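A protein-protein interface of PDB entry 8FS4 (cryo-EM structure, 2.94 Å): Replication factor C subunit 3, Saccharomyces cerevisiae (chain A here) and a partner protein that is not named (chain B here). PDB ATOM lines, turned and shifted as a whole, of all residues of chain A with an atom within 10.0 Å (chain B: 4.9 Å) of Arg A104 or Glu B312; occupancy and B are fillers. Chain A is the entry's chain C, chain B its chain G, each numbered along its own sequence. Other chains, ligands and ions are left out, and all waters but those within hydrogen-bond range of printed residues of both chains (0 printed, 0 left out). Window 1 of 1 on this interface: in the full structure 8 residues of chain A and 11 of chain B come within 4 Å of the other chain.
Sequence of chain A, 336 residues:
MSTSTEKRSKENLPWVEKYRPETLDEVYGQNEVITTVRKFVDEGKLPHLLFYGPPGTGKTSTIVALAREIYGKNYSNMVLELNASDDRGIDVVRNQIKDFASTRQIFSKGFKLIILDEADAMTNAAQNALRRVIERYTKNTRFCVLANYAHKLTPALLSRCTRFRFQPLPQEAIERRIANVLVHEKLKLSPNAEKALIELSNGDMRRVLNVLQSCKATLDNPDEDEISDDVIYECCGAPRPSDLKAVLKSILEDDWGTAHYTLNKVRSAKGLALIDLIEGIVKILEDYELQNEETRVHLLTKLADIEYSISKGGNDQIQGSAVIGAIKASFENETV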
ATOM      1  N   ASN A  74       3.734   0.915 -17.099  1.00  0.00           N
ATOM      2  CA  ASN A  74       3.363   0.913 -18.508  1.00  0.00           C
ATOM      3  C   ASN A  74       1.853   0.990 -18.689  1.00  0.00           C
ATOM      4  O   ASN A  74       1.319   0.579 -19.729  1.00  0.00           O
ATOM      5  CB  ASN A  74       3.928  -0.324 -19.204  1.00  0.00           C
ATOM      6  CG  ASN A  74       4.526  -0.005 -20.561  1.00  0.00           C
ATOM      7  OD1 ASN A  74       4.460   1.130 -21.030  1.00  0.00           O
ATOM      8  ND2 ASN A  74       5.120  -1.005 -21.196  1.00  0.00           N
ATOM      9  N   ASN A  77       1.176   2.905 -21.866  1.00  0.00           N
ATOM     10  CA  ASN A  77       1.436   2.297 -23.160  1.00  0.00           C
ATOM     11  C   ASN A  77       0.626   1.037 -23.400  1.00  0.00           C
ATOM     12  O   ASN A  77       0.566   0.575 -24.544  1.00  0.00           O
ATOM     13  CB  ASN A  77       2.925   1.951 -23.304  1.00  0.00           C
ATOM     14  CG  ASN A  77       3.353   1.805 -24.750  1.00  0.00           C
ATOM     15  OD1 ASN A  77       3.361   2.775 -25.508  1.00  0.00           O
ATOM     16  ND2 ASN A  77       3.713   0.587 -25.140  1.00  0.00           N
ATOM     17  N   MET A  78       0.010   0.471 -22.363  1.00  0.00           N
ATOM     18  CA  MET A  78      -0.768  -0.747 -22.529  1.00  0.00           C
ATOM     19  C   MET A  78      -2.269  -0.523 -22.523  1.00  0.00           C
ATOM     20  O   MET A  78      -3.006  -1.373 -23.029  1.00  0.00           O
ATOM     21  CB  MET A  78      -0.418  -1.761 -21.437  1.00  0.00           C
ATOM     22  CG  MET A  78       0.974  -2.350 -21.565  1.00  0.00           C
ATOM     23  SD  MET A  78       0.997  -3.777 -22.652  1.00  0.00           S
ATOM     24  CE  MET A  78       1.220  -2.927 -24.207  1.00  0.00           C
ATOM     25  N   LYS A  98      -8.580  -0.518 -34.000  1.00  0.00           N
ATOM     26  CA  LYS A  98      -8.070  -1.657 -34.753  1.00  0.00           C
ATOM     27  C   LYS A  98      -6.546  -1.664 -34.790  1.00  0.00           C
ATOM     28  O   LYS A  98      -5.927  -2.728 -34.680  1.00  0.00           O
ATOM     29  CB  LYS A  98      -8.638  -1.653 -36.170  1.00  0.00           C
ATOM     30  CG  LYS A  98      -8.536  -3.002 -36.857  1.00  0.00           C
ATOM     31  CD  LYS A  98      -9.466  -3.101 -38.048  1.00  0.00           C
ATOM     32  CE  LYS A  98      -9.420  -4.488 -38.661  1.00  0.00           C
ATOM     33  NZ  LYS A  98     -10.379  -4.636 -39.786  1.00  0.00           N
ATOM     34  N   ASP A  99      -5.919  -0.494 -34.944  1.00  0.00           N
ATOM     35  CA  ASP A  99      -4.463  -0.448 -34.977  1.00  0.00           C
ATOM     36  C   ASP A  99      -3.866  -0.653 -33.594  1.00  0.00           C
ATOM     37  O   ASP A  99      -2.767  -1.204 -33.474  1.00  0.00           O
ATOM     38  CB  ASP A  99      -3.995   0.878 -35.567  1.00  0.00           C
ATOM     39  CG  ASP A  99      -4.475   1.081 -36.989  1.00  0.00           C
ATOM     40  OD1 ASP A  99      -5.079   0.144 -37.553  1.00  0.00           O
ATOM     41  OD2 ASP A  99      -4.248   2.175 -37.546  1.00  0.00           O
ATOM     42  N   PHE A 100      -4.557  -0.217 -32.542  1.00  0.00           N
ATOM     43  CA  PHE A 100      -4.083  -0.517 -31.198  1.00  0.00           C
ATOM     44  C   PHE A 100      -4.161  -2.012 -30.916  1.00  0.00           C
ATOM     45  O   PHE A 100      -3.282  -2.572 -30.252  1.00  0.00           O
ATOM     46  CB  PHE A 100      -4.890   0.271 -30.169  1.00  0.00           C
ATOM     47  CG  PHE A 100      -4.354   0.170 -28.774  1.00  0.00           C
ATOM     48  CD1 PHE A 100      -3.252   0.909 -28.387  1.00  0.00           C
ATOM     49  CD2 PHE A 100      -4.954  -0.659 -27.847  1.00  0.00           C
ATOM     50  CE1 PHE A 100      -2.760   0.818 -27.103  1.00  0.00           C
ATOM     51  CE2 PHE A 100      -4.465  -0.752 -26.563  1.00  0.00           C
ATOM     52  CZ  PHE A 100      -3.367  -0.014 -26.190  1.00  0.00           C
ATOM     53  N   ALA A 101      -5.205  -2.676 -31.417  1.00  0.00           N
ATOM     54  CA  ALA A 101      -5.375  -4.101 -31.151  1.00  0.00           C
ATOM     55  C   ALA A 101      -4.446  -4.962 -32.000  1.00  0.00           C
ATOM     56  O   ALA A 101      -3.939  -5.983 -31.524  1.00  0.00           O
ATOM     57  CB  ALA A 101      -6.830  -4.503 -31.388  1.00  0.00           C
ATOM     58  N   SER A 102      -4.213  -4.577 -33.255  1.00  0.00           N
ATOM     59  CA  SER A 102      -3.410  -5.413 -34.141  1.00  0.00           C
ATOM     60  C   SER A 102      -1.939  -5.401 -33.741  1.00  0.00           C
ATOM     61  O   SER A 102      -1.266  -6.436 -33.802  1.00  0.00           O
ATOM     62  CB  SER A 102      -3.574  -4.947 -35.586  1.00  0.00           C
ATOM     63  OG  SER A 102      -4.941  -4.770 -35.908  1.00  0.00           O
ATOM     64  N   THR A 103      -1.406  -4.223 -33.409  1.00  0.00           N
ATOM     65  CA  THR A 103       0.024  -4.061 -33.043  1.00  0.00           C
ATOM     66  C   THR A 103       0.376  -5.015 -31.904  1.00  0.00           C
ATOM     67  O   THR A 103      -0.556  -5.601 -31.325  1.00  0.00           O
ATOM     68  CB  THR A 103       0.326  -2.613 -32.655  1.00  0.00           C
ATOM     69  OG1 THR A 103      -0.758  -2.157 -31.847  1.00  0.00           O
ATOM     70  CG2 THR A 103       0.497  -1.707 -33.853  1.00  0.00           C
ATOM     71  N   ARG A 104       1.668  -5.125 -31.573  1.00  0.00           N
ATOM     72  CA  ARG A 104       2.127  -6.011 -30.470  1.00  0.00           C
ATOM     73  C   ARG A 104       2.271  -5.191 -29.187  1.00  0.00           C
ATOM     74  O   ARG A 104       2.402  -3.959 -29.292  1.00  0.00           O
ATOM     75  CB  ARG A 104       3.467  -6.655 -30.834  1.00  0.00           C
ATOM     76  CG  ARG A 104       3.959  -7.688 -29.832  1.00  0.00           C
ATOM     77  CD  ARG A 104       4.116  -9.051 -30.478  1.00  0.00           C
ATOM     78  NE  ARG A 104       5.063  -9.025 -31.582  1.00  0.00           N
ATOM     79  CZ  ARG A 104       6.367  -9.238 -31.456  1.00  0.00           C
ATOM     80  NH1 ARG A 104       6.884  -9.494 -30.267  1.00  0.00           N
ATOM     81  NH2 ARG A 104       7.150  -9.196 -32.519  1.00  0.00           N
ATOM     82  N   GLN A 105       2.270  -5.850 -28.027  1.00  0.00           N
ATOM     83  CA  GLN A 105       2.322  -5.126 -26.727  1.00  0.00           C
ATOM     84  C   GLN A 105       3.755  -5.072 -26.200  1.00  0.00           C
ATOM     85  O   GLN A 105       3.911  -4.935 -24.973  1.00  0.00           O
ATOM     86  CB  GLN A 105       1.469  -5.852 -25.689  1.00  0.00           C
ATOM     87  CG  GLN A 105       1.903  -7.291 -25.456  1.00  0.00           C
ATOM     88  CD  GLN A 105       1.256  -8.252 -26.423  1.00  0.00           C
ATOM     89  OE1 GLN A 105       1.682  -8.394 -27.567  1.00  0.00           O
ATOM     90  NE2 GLN A 105       0.217  -8.927 -25.962  1.00  0.00           N
ATOM     91  N   ILE A 106       4.752  -5.217 -27.076  1.00  0.00           N
ATOM     92  CA  ILE A 106       6.176  -5.262 -26.625  1.00  0.00           C
ATOM     93  C   ILE A 106       6.289  -6.317 -25.515  1.00  0.00           C
ATOM     94  O   ILE A 106       7.227  -6.214 -24.696  1.00  0.00           O
ATOM     95  CB  ILE A 106       6.682  -3.867 -26.192  1.00  0.00           C
ATOM     96  CG1 ILE A 106       6.248  -3.488 -24.773  1.00  0.00           C
ATOM     97  CG2 ILE A 106       6.273  -2.810 -27.207  1.00  0.00           C
ATOM     98  CD1 ILE A 106       6.577  -2.066 -24.388  1.00  0.00           C
ATOM     99  N   PHE A 107       5.365  -7.286 -25.490  1.00  0.00           N
ATOM    100  CA  PHE A 107       5.414  -8.392 -24.495  1.00  0.00           C
ATOM    101  C   PHE A 107       5.116  -7.861 -23.088  1.00  0.00           C
ATOM    102  O   PHE A 107       5.002  -8.677 -22.154  1.00  0.00           O
ATOM    103  CB  PHE A 107       6.769  -9.104 -24.566  1.00  0.00           C
ATOM    104  CG  PHE A 107       7.101  -9.945 -23.360  1.00  0.00           C
ATOM    105  CD1 PHE A 107       6.521 -11.190 -23.180  1.00  0.00           C
ATOM    106  CD2 PHE A 107       7.985  -9.484 -22.397  1.00  0.00           C
ATOM    107  CE1 PHE A 107       6.822 -11.959 -22.066  1.00  0.00           C
ATOM    108  CE2 PHE A 107       8.285 -10.254 -21.284  1.00  0.00           C
ATOM    109  CZ  PHE A 107       7.704 -11.489 -21.121  1.00  0.00           C
ATOM    110  N   SER A 108       4.953  -6.545 -22.940  1.00  0.00           N
ATOM    111  CA  SER A 108       4.771  -5.960 -21.584  1.00  0.00           C
ATOM    112  C   SER A 108       3.439  -6.391 -20.960  1.00  0.00           C
ATOM    113  O   SER A 108       2.392  -6.140 -21.584  1.00  0.00           O
ATOM    114  CB  SER A 108       4.895  -4.458 -21.621  1.00  0.00           C
ATOM    115  OG  SER A 108       4.584  -3.897 -20.355  1.00  0.00           O
ATOM    116  N   LYS A 109       3.483  -7.027 -19.787  1.00  0.00           N
ATOM    117  CA  LYS A 109       2.242  -7.397 -19.046  1.00  0.00           C
ATOM    118  C   LYS A 109       1.238  -8.126 -19.947  1.00  0.00           C
ATOM    119  O   LYS A 109       0.034  -7.818 -19.846  1.00  0.00           O
ATOM    120  CB  LYS A 109       1.622  -6.142 -18.427  1.00  0.00           C
ATOM    121  CG  LYS A 109       2.600  -5.254 -17.672  1.00  0.00           C
ATOM    122  CD  LYS A 109       3.369  -6.001 -16.605  1.00  0.00           C
ATOM    123  CE  LYS A 109       4.487  -5.183 -15.996  1.00  0.00           C
ATOM    124  NZ  LYS A 109       5.223  -5.946 -14.962  1.00  0.00           N
ATOM    125  N   GLY A 110       1.699  -9.060 -20.779  1.00  0.00           N
ATOM    126  CA  GLY A 110       0.765  -9.871 -21.583  1.00  0.00           C
ATOM    127  C   GLY A 110      -0.138  -9.052 -22.486  1.00  0.00           C
ATOM    128  O   GLY A 110       0.396  -8.280 -23.296  1.00  0.00           O
ATOM    129  N   PHE A 111      -1.458  -9.197 -22.346  1.00  0.00           N
ATOM    130  CA  PHE A 111      -2.414  -8.535 -23.273  1.00  0.00           C
ATOM    131  C   PHE A 111      -2.497  -7.024 -23.058  1.00  0.00           C
ATOM    132  O   PHE A 111      -2.113  -6.547 -21.975  1.00  0.00           O
ATOM    133  CB  PHE A 111      -3.812  -9.125 -23.081  1.00  0.00           C
ATOM    134  CG  PHE A 111      -4.363  -8.959 -21.688  1.00  0.00           C
ATOM    135  CD1 PHE A 111      -5.049  -7.811 -21.328  1.00  0.00           C
ATOM    136  CD2 PHE A 111      -4.188  -9.948 -20.734  1.00  0.00           C
ATOM    137  CE1 PHE A 111      -5.551  -7.658 -20.045  1.00  0.00           C
ATOM    138  CE2 PHE A 111      -4.692  -9.795 -19.453  1.00  0.00           C
ATOM    139  CZ  PHE A 111      -5.371  -8.650 -19.111  1.00  0.00           C
ATOM    140  N   LYS A 112      -2.988  -6.300 -24.068  1.00  0.00           N
ATOM    141  CA  LYS A 112      -3.210  -4.840 -23.936  1.00  0.00           C
ATOM    142  C   LYS A 112      -4.658  -4.681 -23.483  1.00  0.00           C
ATOM    143  O   LYS A 112      -5.408  -5.639 -23.666  1.00  0.00           O
ATOM    144  CB  LYS A 112      -2.997  -4.113 -25.263  1.00  0.00           C
ATOM    145  CG  LYS A 112      -1.779  -4.531 -26.071  1.00  0.00           C
ATOM    146  CD  LYS A 112      -1.776  -3.914 -27.451  1.00  0.00           C
ATOM    147  CE  LYS A 112      -0.464  -4.082 -28.180  1.00  0.00           C
ATOM    148  NZ  LYS A 112      -0.442  -3.290 -29.431  1.00  0.00           N
ATOM    149  N   LEU A 113      -5.045  -3.541 -22.918  1.00  0.00           N
ATOM    150  CA  LEU A 113      -6.395  -3.291 -22.438  1.00  0.00           C
ATOM    151  C   LEU A 113      -6.958  -2.069 -23.145  1.00  0.00           C
ATOM    152  O   LEU A 113      -6.234  -1.104 -23.404  1.00  0.00           O
ATOM    153  CB  LEU A 113      -6.405  -3.085 -20.919  1.00  0.00           C
ATOM    154  CG  LEU A 113      -7.624  -2.407 -20.296  1.00  0.00           C
ATOM    155  CD1 LEU A 113      -8.853  -3.278 -20.421  1.00  0.00           C
ATOM    156  CD2 LEU A 113      -7.355  -2.088 -18.842  1.00  0.00           C
ATOM    157  N   TYR A 137      -9.069 -10.018 -31.952  1.00  0.00           N
ATOM    158  CA  TYR A 137      -7.835  -9.739 -31.232  1.00  0.00           C
ATOM    159  C   TYR A 137      -7.984  -9.971 -29.735  1.00  0.00           C
ATOM    160  O   TYR A 137      -7.310  -9.316 -28.934  1.00  0.00           O
ATOM    161  CB  TYR A 137      -7.385  -8.309 -31.516  1.00  0.00           C
ATOM    162  CG  TYR A 137      -7.336  -7.994 -32.989  1.00  0.00           C
ATOM    163  CD1 TYR A 137      -6.276  -8.421 -33.774  1.00  0.00           C
ATOM    164  CD2 TYR A 137      -8.353  -7.279 -33.600  1.00  0.00           C
ATOM    165  CE1 TYR A 137      -6.228  -8.140 -35.122  1.00  0.00           C
ATOM    166  CE2 TYR A 137      -8.314  -6.993 -34.947  1.00  0.00           C
ATOM    167  CZ  TYR A 137      -7.249  -7.426 -35.703  1.00  0.00           C
ATOM    168  OH  TYR A 137      -7.206  -7.142 -37.047  1.00  0.00           O
ATOM    169  N   LYS A 139      -6.890 -12.448 -28.336  1.00  0.00           N
ATOM    170  CA  LYS A 139      -5.648 -13.091 -27.935  1.00  0.00           C
ATOM    171  C   LYS A 139      -4.593 -12.077 -27.516  1.00  0.00           C
ATOM    172  O   LYS A 139      -3.672 -12.423 -26.768  1.00  0.00           O
ATOM    173  CB  LYS A 139      -5.119 -13.955 -29.076  1.00  0.00           C
ATOM    174  CG  LYS A 139      -4.793 -13.168 -30.348  1.00  0.00           C
ATOM    175  CD  LYS A 139      -4.318 -14.045 -31.508  1.00  0.00           C
ATOM    176  CE  LYS A 139      -3.469 -15.244 -31.088  1.00  0.00           C
ATOM    177  NZ  LYS A 139      -2.371 -14.920 -30.118  1.00  0.00           N
ATOM    178  N   ASN A 140      -4.709 -10.835 -27.983  1.00  0.00           N
ATOM    179  CA  ASN A 140      -3.766  -9.779 -27.641  1.00  0.00           C
ATOM    180  C   ASN A 140      -4.364  -8.675 -26.785  1.00  0.00           C
ATOM    181  O   ASN A 140      -3.633  -8.056 -26.011  1.00  0.00           O
ATOM    182  CB  ASN A 140      -3.191  -9.150 -28.915  1.00  0.00           C
ATOM    183  CG  ASN A 140      -2.096  -8.144 -28.623  1.00  0.00           C
ATOM    184  OD1 ASN A 140      -2.368  -6.984 -28.319  1.00  0.00           O
ATOM    185  ND2 ASN A 140      -0.847  -8.588 -28.708  1.00  0.00           N
ATOM    186  N   THR A 141      -5.665  -8.413 -26.897  1.00  0.00           N
ATOM    187  CA  THR A 141      -6.306  -7.315 -26.189  1.00  0.00           C
ATOM    188  C   THR A 141      -7.548  -7.797 -25.457  1.00  0.00           C
ATOM    189  O   THR A 141      -8.153  -8.807 -25.821  1.00  0.00           O
ATOM    190  CB  THR A 141      -6.709  -6.188 -27.141  1.00  0.00           C
ATOM    191  OG1 THR A 141      -7.745  -6.648 -28.016  1.00  0.00           O
ATOM    192  CG2 THR A 141      -5.526  -5.729 -27.960  1.00  0.00           C
ATOM    193  N   ILE B 234      11.493 -11.593 -39.661  1.00  0.00           N
ATOM    194  CA  ILE B 234      10.325 -11.174 -40.423  1.00  0.00           C
ATOM    195  C   ILE B 234       9.579 -10.112 -39.628  1.00  0.00           C
ATOM    196  O   ILE B 234       9.301 -10.299 -38.437  1.00  0.00           O
ATOM    197  CB  ILE B 234       9.409 -12.369 -40.737  1.00  0.00           C
ATOM    198  CG1 ILE B 234      10.171 -13.463 -41.489  1.00  0.00           C
ATOM    199  CG2 ILE B 234       8.230 -11.922 -41.555  1.00  0.00           C
ATOM    200  CD1 ILE B 234      11.053 -12.966 -42.600  1.00  0.00           C
ATOM    201  N   GLY B 235       9.255  -9.001 -40.288  1.00  0.00           N
ATOM    202  CA  GLY B 235       8.500  -7.930 -39.668  1.00  0.00           C
ATOM    203  C   GLY B 235       7.221  -7.605 -40.414  1.00  0.00           C
ATOM    204  O   GLY B 235       7.263  -7.154 -41.562  1.00  0.00           O
ATOM    205  N   PHE B 236       6.076  -7.830 -39.772  1.00  0.00           N
ATOM    206  CA  PHE B 236       4.769  -7.560 -40.363  1.00  0.00           C
ATOM    207  C   PHE B 236       4.284  -6.203 -39.859  1.00  0.00           C
ATOM    208  O   PHE B 236       3.880  -6.073 -38.700  1.00  0.00           O
ATOM    209  CB  PHE B 236       3.779  -8.668 -40.006  1.00  0.00           C
ATOM    210  CG  PHE B 236       2.435  -8.525 -40.667  1.00  0.00           C
ATOM    211  CD1 PHE B 236       2.324  -8.031 -41.956  1.00  0.00           C
ATOM    212  CD2 PHE B 236       1.282  -8.892 -39.995  1.00  0.00           C
ATOM    213  CE1 PHE B 236       1.090  -7.903 -42.558  1.00  0.00           C
ATOM    214  CE2 PHE B 236       0.045  -8.765 -40.594  1.00  0.00           C
ATOM    215  CZ  PHE B 236      -0.050  -8.270 -41.878  1.00  0.00           C
ATOM    216  N   PHE B 237       4.317  -5.200 -40.734  1.00  0.00           N
ATOM    217  CA  PHE B 237       3.993  -3.828 -40.368  1.00  0.00           C
ATOM    218  C   PHE B 237       2.840  -3.308 -41.213  1.00  0.00           C
ATOM    219  O   PHE B 237       2.702  -3.656 -42.390  1.00  0.00           O
ATOM    220  CB  PHE B 237       5.205  -2.909 -40.544  1.00  0.00           C
ATOM    221  CG  PHE B 237       6.371  -3.276 -39.677  1.00  0.00           C
ATOM    222  CD1 PHE B 237       6.382  -2.942 -38.334  1.00  0.00           C
ATOM    223  CD2 PHE B 237       7.451  -3.959 -40.203  1.00  0.00           C
ATOM    224  CE1 PHE B 237       7.452  -3.281 -37.532  1.00  0.00           C
ATOM    225  CE2 PHE B 237       8.523  -4.300 -39.406  1.00  0.00           C
ATOM    226  CZ  PHE B 237       8.521  -3.962 -38.069  1.00  0.00           C
ATOM    227  N   VAL B 261      13.283  -8.477 -30.981  1.00  0.00           N
ATOM    228  CA  VAL B 261      12.308  -9.568 -31.001  1.00  0.00           C
ATOM    229  C   VAL B 261      10.964  -9.166 -30.419  1.00  0.00           C
ATOM    230  O   VAL B 261       9.987  -9.908 -30.582  1.00  0.00           O
ATOM    231  CB  VAL B 261      12.791 -10.814 -30.234  1.00  0.00           C
ATOM    232  CG1 VAL B 261      14.070 -11.363 -30.853  1.00  0.00           C
ATOM    233  CG2 VAL B 261      12.981 -10.508 -28.761  1.00  0.00           C
ATOM    234  N   HIS B 262      10.880  -8.021 -29.741  1.00  0.00           N
ATOM    235  CA  HIS B 262       9.603  -7.551 -29.220  1.00  0.00           C
ATOM    236  C   HIS B 262       8.720  -6.934 -30.296  1.00  0.00           C
ATOM    237  O   HIS B 262       7.564  -6.608 -30.010  1.00  0.00           O
ATOM    238  CB  HIS B 262       9.827  -6.531 -28.100  1.00  0.00           C
ATOM    239  CG  HIS B 262      10.756  -7.005 -27.026  1.00  0.00           C
ATOM    240  ND1 HIS B 262      10.390  -7.946 -26.088  1.00  0.00           N
ATOM    241  CD2 HIS B 262      12.031  -6.661 -26.735  1.00  0.00           C
ATOM    242  CE1 HIS B 262      11.403  -8.165 -25.268  1.00  0.00           C
ATOM    243  NE2 HIS B 262      12.411  -7.397 -25.638  1.00  0.00           N
ATOM    244  N   GLY B 263       9.232  -6.763 -31.512  1.00  0.00           N
ATOM    245  CA  GLY B 263       8.433  -6.243 -32.602  1.00  0.00           C
ATOM    246  C   GLY B 263       8.394  -4.732 -32.646  1.00  0.00           C
ATOM    247  O   GLY B 263       7.321  -4.137 -32.786  1.00  0.00           O
ATOM    248  N   VAL B 264       9.558  -4.098 -32.525  1.00  0.00           N
ATOM    249  CA  VAL B 264       9.684  -2.648 -32.605  1.00  0.00           C
ATOM    250  C   VAL B 264      10.746  -2.331 -33.646  1.00  0.00           C
ATOM    251  O   VAL B 264      11.899  -2.758 -33.507  1.00  0.00           O
ATOM    252  CB  VAL B 264      10.050  -2.025 -31.247  1.00  0.00           C
ATOM    253  CG1 VAL B 264      10.348  -0.540 -31.395  1.00  0.00           C
ATOM    254  CG2 VAL B 264       8.929  -2.245 -30.250  1.00  0.00           C
ATOM    255  N   MET B 310       8.388   2.090 -34.600  1.00  0.00           N
ATOM    256  CA  MET B 310       7.201   1.498 -35.194  1.00  0.00           C
ATOM    257  C   MET B 310       6.935   0.146 -34.554  1.00  0.00           C
ATOM    258  O   MET B 310       7.867  -0.625 -34.306  1.00  0.00           O
ATOM    259  CB  MET B 310       7.388   1.348 -36.706  1.00  0.00           C
ATOM    260  CG  MET B 310       6.128   0.999 -37.476  1.00  0.00           C
ATOM    261  SD  MET B 310       6.002   1.758 -39.114  1.00  0.00           S
ATOM    262  CE  MET B 310       7.714   2.057 -39.569  1.00  0.00           C
ATOM    263  N   LEU B 311       5.665  -0.134 -34.282  1.00  0.00           N
ATOM    264  CA  LEU B 311       5.272  -1.389 -33.663  1.00  0.00           C
ATOM    265  C   LEU B 311       4.890  -2.413 -34.724  1.00  0.00           C
ATOM    266  O   LEU B 311       4.465  -2.065 -35.829  1.00  0.00           O
ATOM    267  CB  LEU B 311       4.102  -1.180 -32.701  1.00  0.00           C
ATOM    268  CG  LEU B 311       4.463  -1.119 -31.216  1.00  0.00           C
ATOM    269  CD1 LEU B 311       3.238  -0.777 -30.390  1.00  0.00           C
ATOM    270  CD2 LEU B 311       5.069  -2.428 -30.740  1.00  0.00           C
ATOM    271  N   GLU B 312       5.044  -3.685 -34.373  1.00  0.00           N
ATOM    272  CA  GLU B 312       4.785  -4.792 -35.280  1.00  0.00           C
ATOM    273  C   GLU B 312       3.402  -5.378 -35.024  1.00  0.00           C
ATOM    274  O   GLU B 312       2.909  -5.391 -33.893  1.00  0.00           O
ATOM    275  CB  GLU B 312       5.848  -5.880 -35.121  1.00  0.00           C
ATOM    276  CG  GLU B 312       6.117  -6.671 -36.395  1.00  0.00           C
ATOM    277  CD  GLU B 312       6.326  -8.156 -36.150  1.00  0.00           C
ATOM    278  OE1 GLU B 312       6.028  -8.638 -35.037  1.00  0.00           O
ATOM    279  OE2 GLU B 312       6.780  -8.848 -37.083  1.00  0.00           O
ATOM    280  N   LYS B 313       2.781  -5.868 -36.092  1.00  0.00           N
ATOM    281  CA  LYS B 313       1.439  -6.417 -36.007  1.00  0.00           C
ATOM    282  C   LYS B 313       1.458  -7.793 -35.344  1.00  0.00           C
ATOM    283  O   LYS B 313       2.511  -8.394 -35.116  1.00  0.00           O
ATOM    284  CB  LYS B 313       0.812  -6.511 -37.397  1.00  0.00           C
ATOM    285  CG  LYS B 313       0.666  -5.172 -38.105  1.00  0.00           C
ATOM    286  CD  LYS B 313      -0.750  -4.619 -37.999  1.00  0.00           C
ATOM    287  CE  LYS B 313      -1.762  -5.441 -38.785  1.00  0.00           C
ATOM    288  NZ  LYS B 313      -1.406  -5.568 -40.224  1.00  0.00           N
ATOM    289  N   GLU B 314       0.261  -8.287 -35.022  1.00  0.00           N
ATOM    290  CA  GLU B 314       0.142  -9.607 -34.410  1.00  0.00           C
ATOM    291  C   GLU B 314       0.518 -10.713 -35.388  1.00  0.00           C
ATOM    292  O   GLU B 314       1.210 -11.669 -35.015  1.00  0.00           O
ATOM    293  CB  GLU B 314      -1.288  -9.821 -33.905  1.00  0.00           C
ATOM    294  CG  GLU B 314      -1.589  -9.360 -32.471  1.00  0.00           C
ATOM    295  CD  GLU B 314      -0.392  -9.419 -31.540  1.00  0.00           C
ATOM    296  OE1 GLU B 314      -0.075 -10.522 -31.047  1.00  0.00           O
ATOM    297  OE2 GLU B 314       0.230  -8.363 -31.300  1.00  0.00           O
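Among the printed residues, merely in contact across the chains: Ser A102 with Lys B313, Thr A103 with Leu B311, Thr A103 with Glu B312, Arg A104 with Leu B311, Arg A104 with Glu B314, Ile A106 with His B262 and Ile A106 with Leu B311.
Glu B312 touches two residues of chain A.
No residue of chain A comes within 4 Å of Gly B235.
Gly B263 touches just one residue of chain A: Arg A104 (3.2 Å).
Printed residues of chain A within 4 Å of Lys B313: Ser A102.
Of the printed residues of chain A, His B262 touches Arg A104 and Ile A106.
Phe A111 touches none of the printed residues of chain B.
Ala A101 touches none of the printed residues of chain B.
The nearest residue of chain B that does not touch Arg A104 is Lys B313 (4.4 Å).
The nearest residue of chain A that does not touch Glu B312 is Ser A102 (4.3 Å).
The nearest printed residue of chain B that does not touch Asn A140 is Lys B313 (7.1 Å).
The side-chain hydroxyl (OG) of Ser A102 sits at hydrogen-bond distance from the side-chain hydroxyl (OH) of Tyr A137.
The side-chain amino group (NZ) of Lys A112 sits at hydrogen-bond distance from the side-chain hydroxyl (OG1) of Thr A103.
The side-chain amide oxygen (OE1) of Gln A105 is in hydrogen-bond range of the side-chain amide nitrogen (ND2) of Asn A140 (2.8 Å).
N of Phe B236 lies within hydrogen-bond range of OE2 of Glu B312 (3.0 Å).
The backbone NH of Lys B313 is in hydrogen-bond range of the backbone carbonyl oxygen of Phe B236, 2.8 Å away.
O of Gly B263 is in hydrogen-bond range of N of Glu B312 (2.8 Å).
Of the 23 printed residues of chain A, 5 touch a printed residue of chain B.
Of the 13 printed residues of chain B, 7 touch a printed residue of chain A.
Printed residues of chain B that touch a printed residue of chain A: Val B261, His B262, Gly B263, Leu B311, Glu B312, Lys B313 and Glu B314.
Hydrophobic or aromatic side chains of chain B that line the printed part of chain A: His B262 and Leu B311.
Among the printed residues, 14 pairs touch across the chains.
Among the printed residues, Asp or Glu carboxylates within 4 Å of a Lys or Arg side-chain nitrogen of the other chain: Arg A104 with Glu B312.
N of Glu B314 sits at hydrogen-bond distance from O of Ser A102 (2.7 Å).
The guanidinium group (NH1) of Arg A104 sits at hydrogen-bond distance from the backbone carbonyl oxygen (O) of Val B261 (3.1 Å).
NH1 of Arg A104 is in hydrogen-bond range of O of His B262 (3.0 Å).
OE1 of Glu B312 is in salt-bridge range of NH2 of Arg A104, at 2.8 Å.
ND2 of Asn A140 lies within hydrogen-bond range of OE2 of Glu B314 (2.8 Å).
The backbone carbonyl oxygen (O) of Thr A103 sits close to the side-chain carboxylate (OE2) of Glu B314 (2.9 Å).
The guanidinium group (NH2) of Arg A104 lies close to the backbone NH (N) of Gly B263 (3.4 Å).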
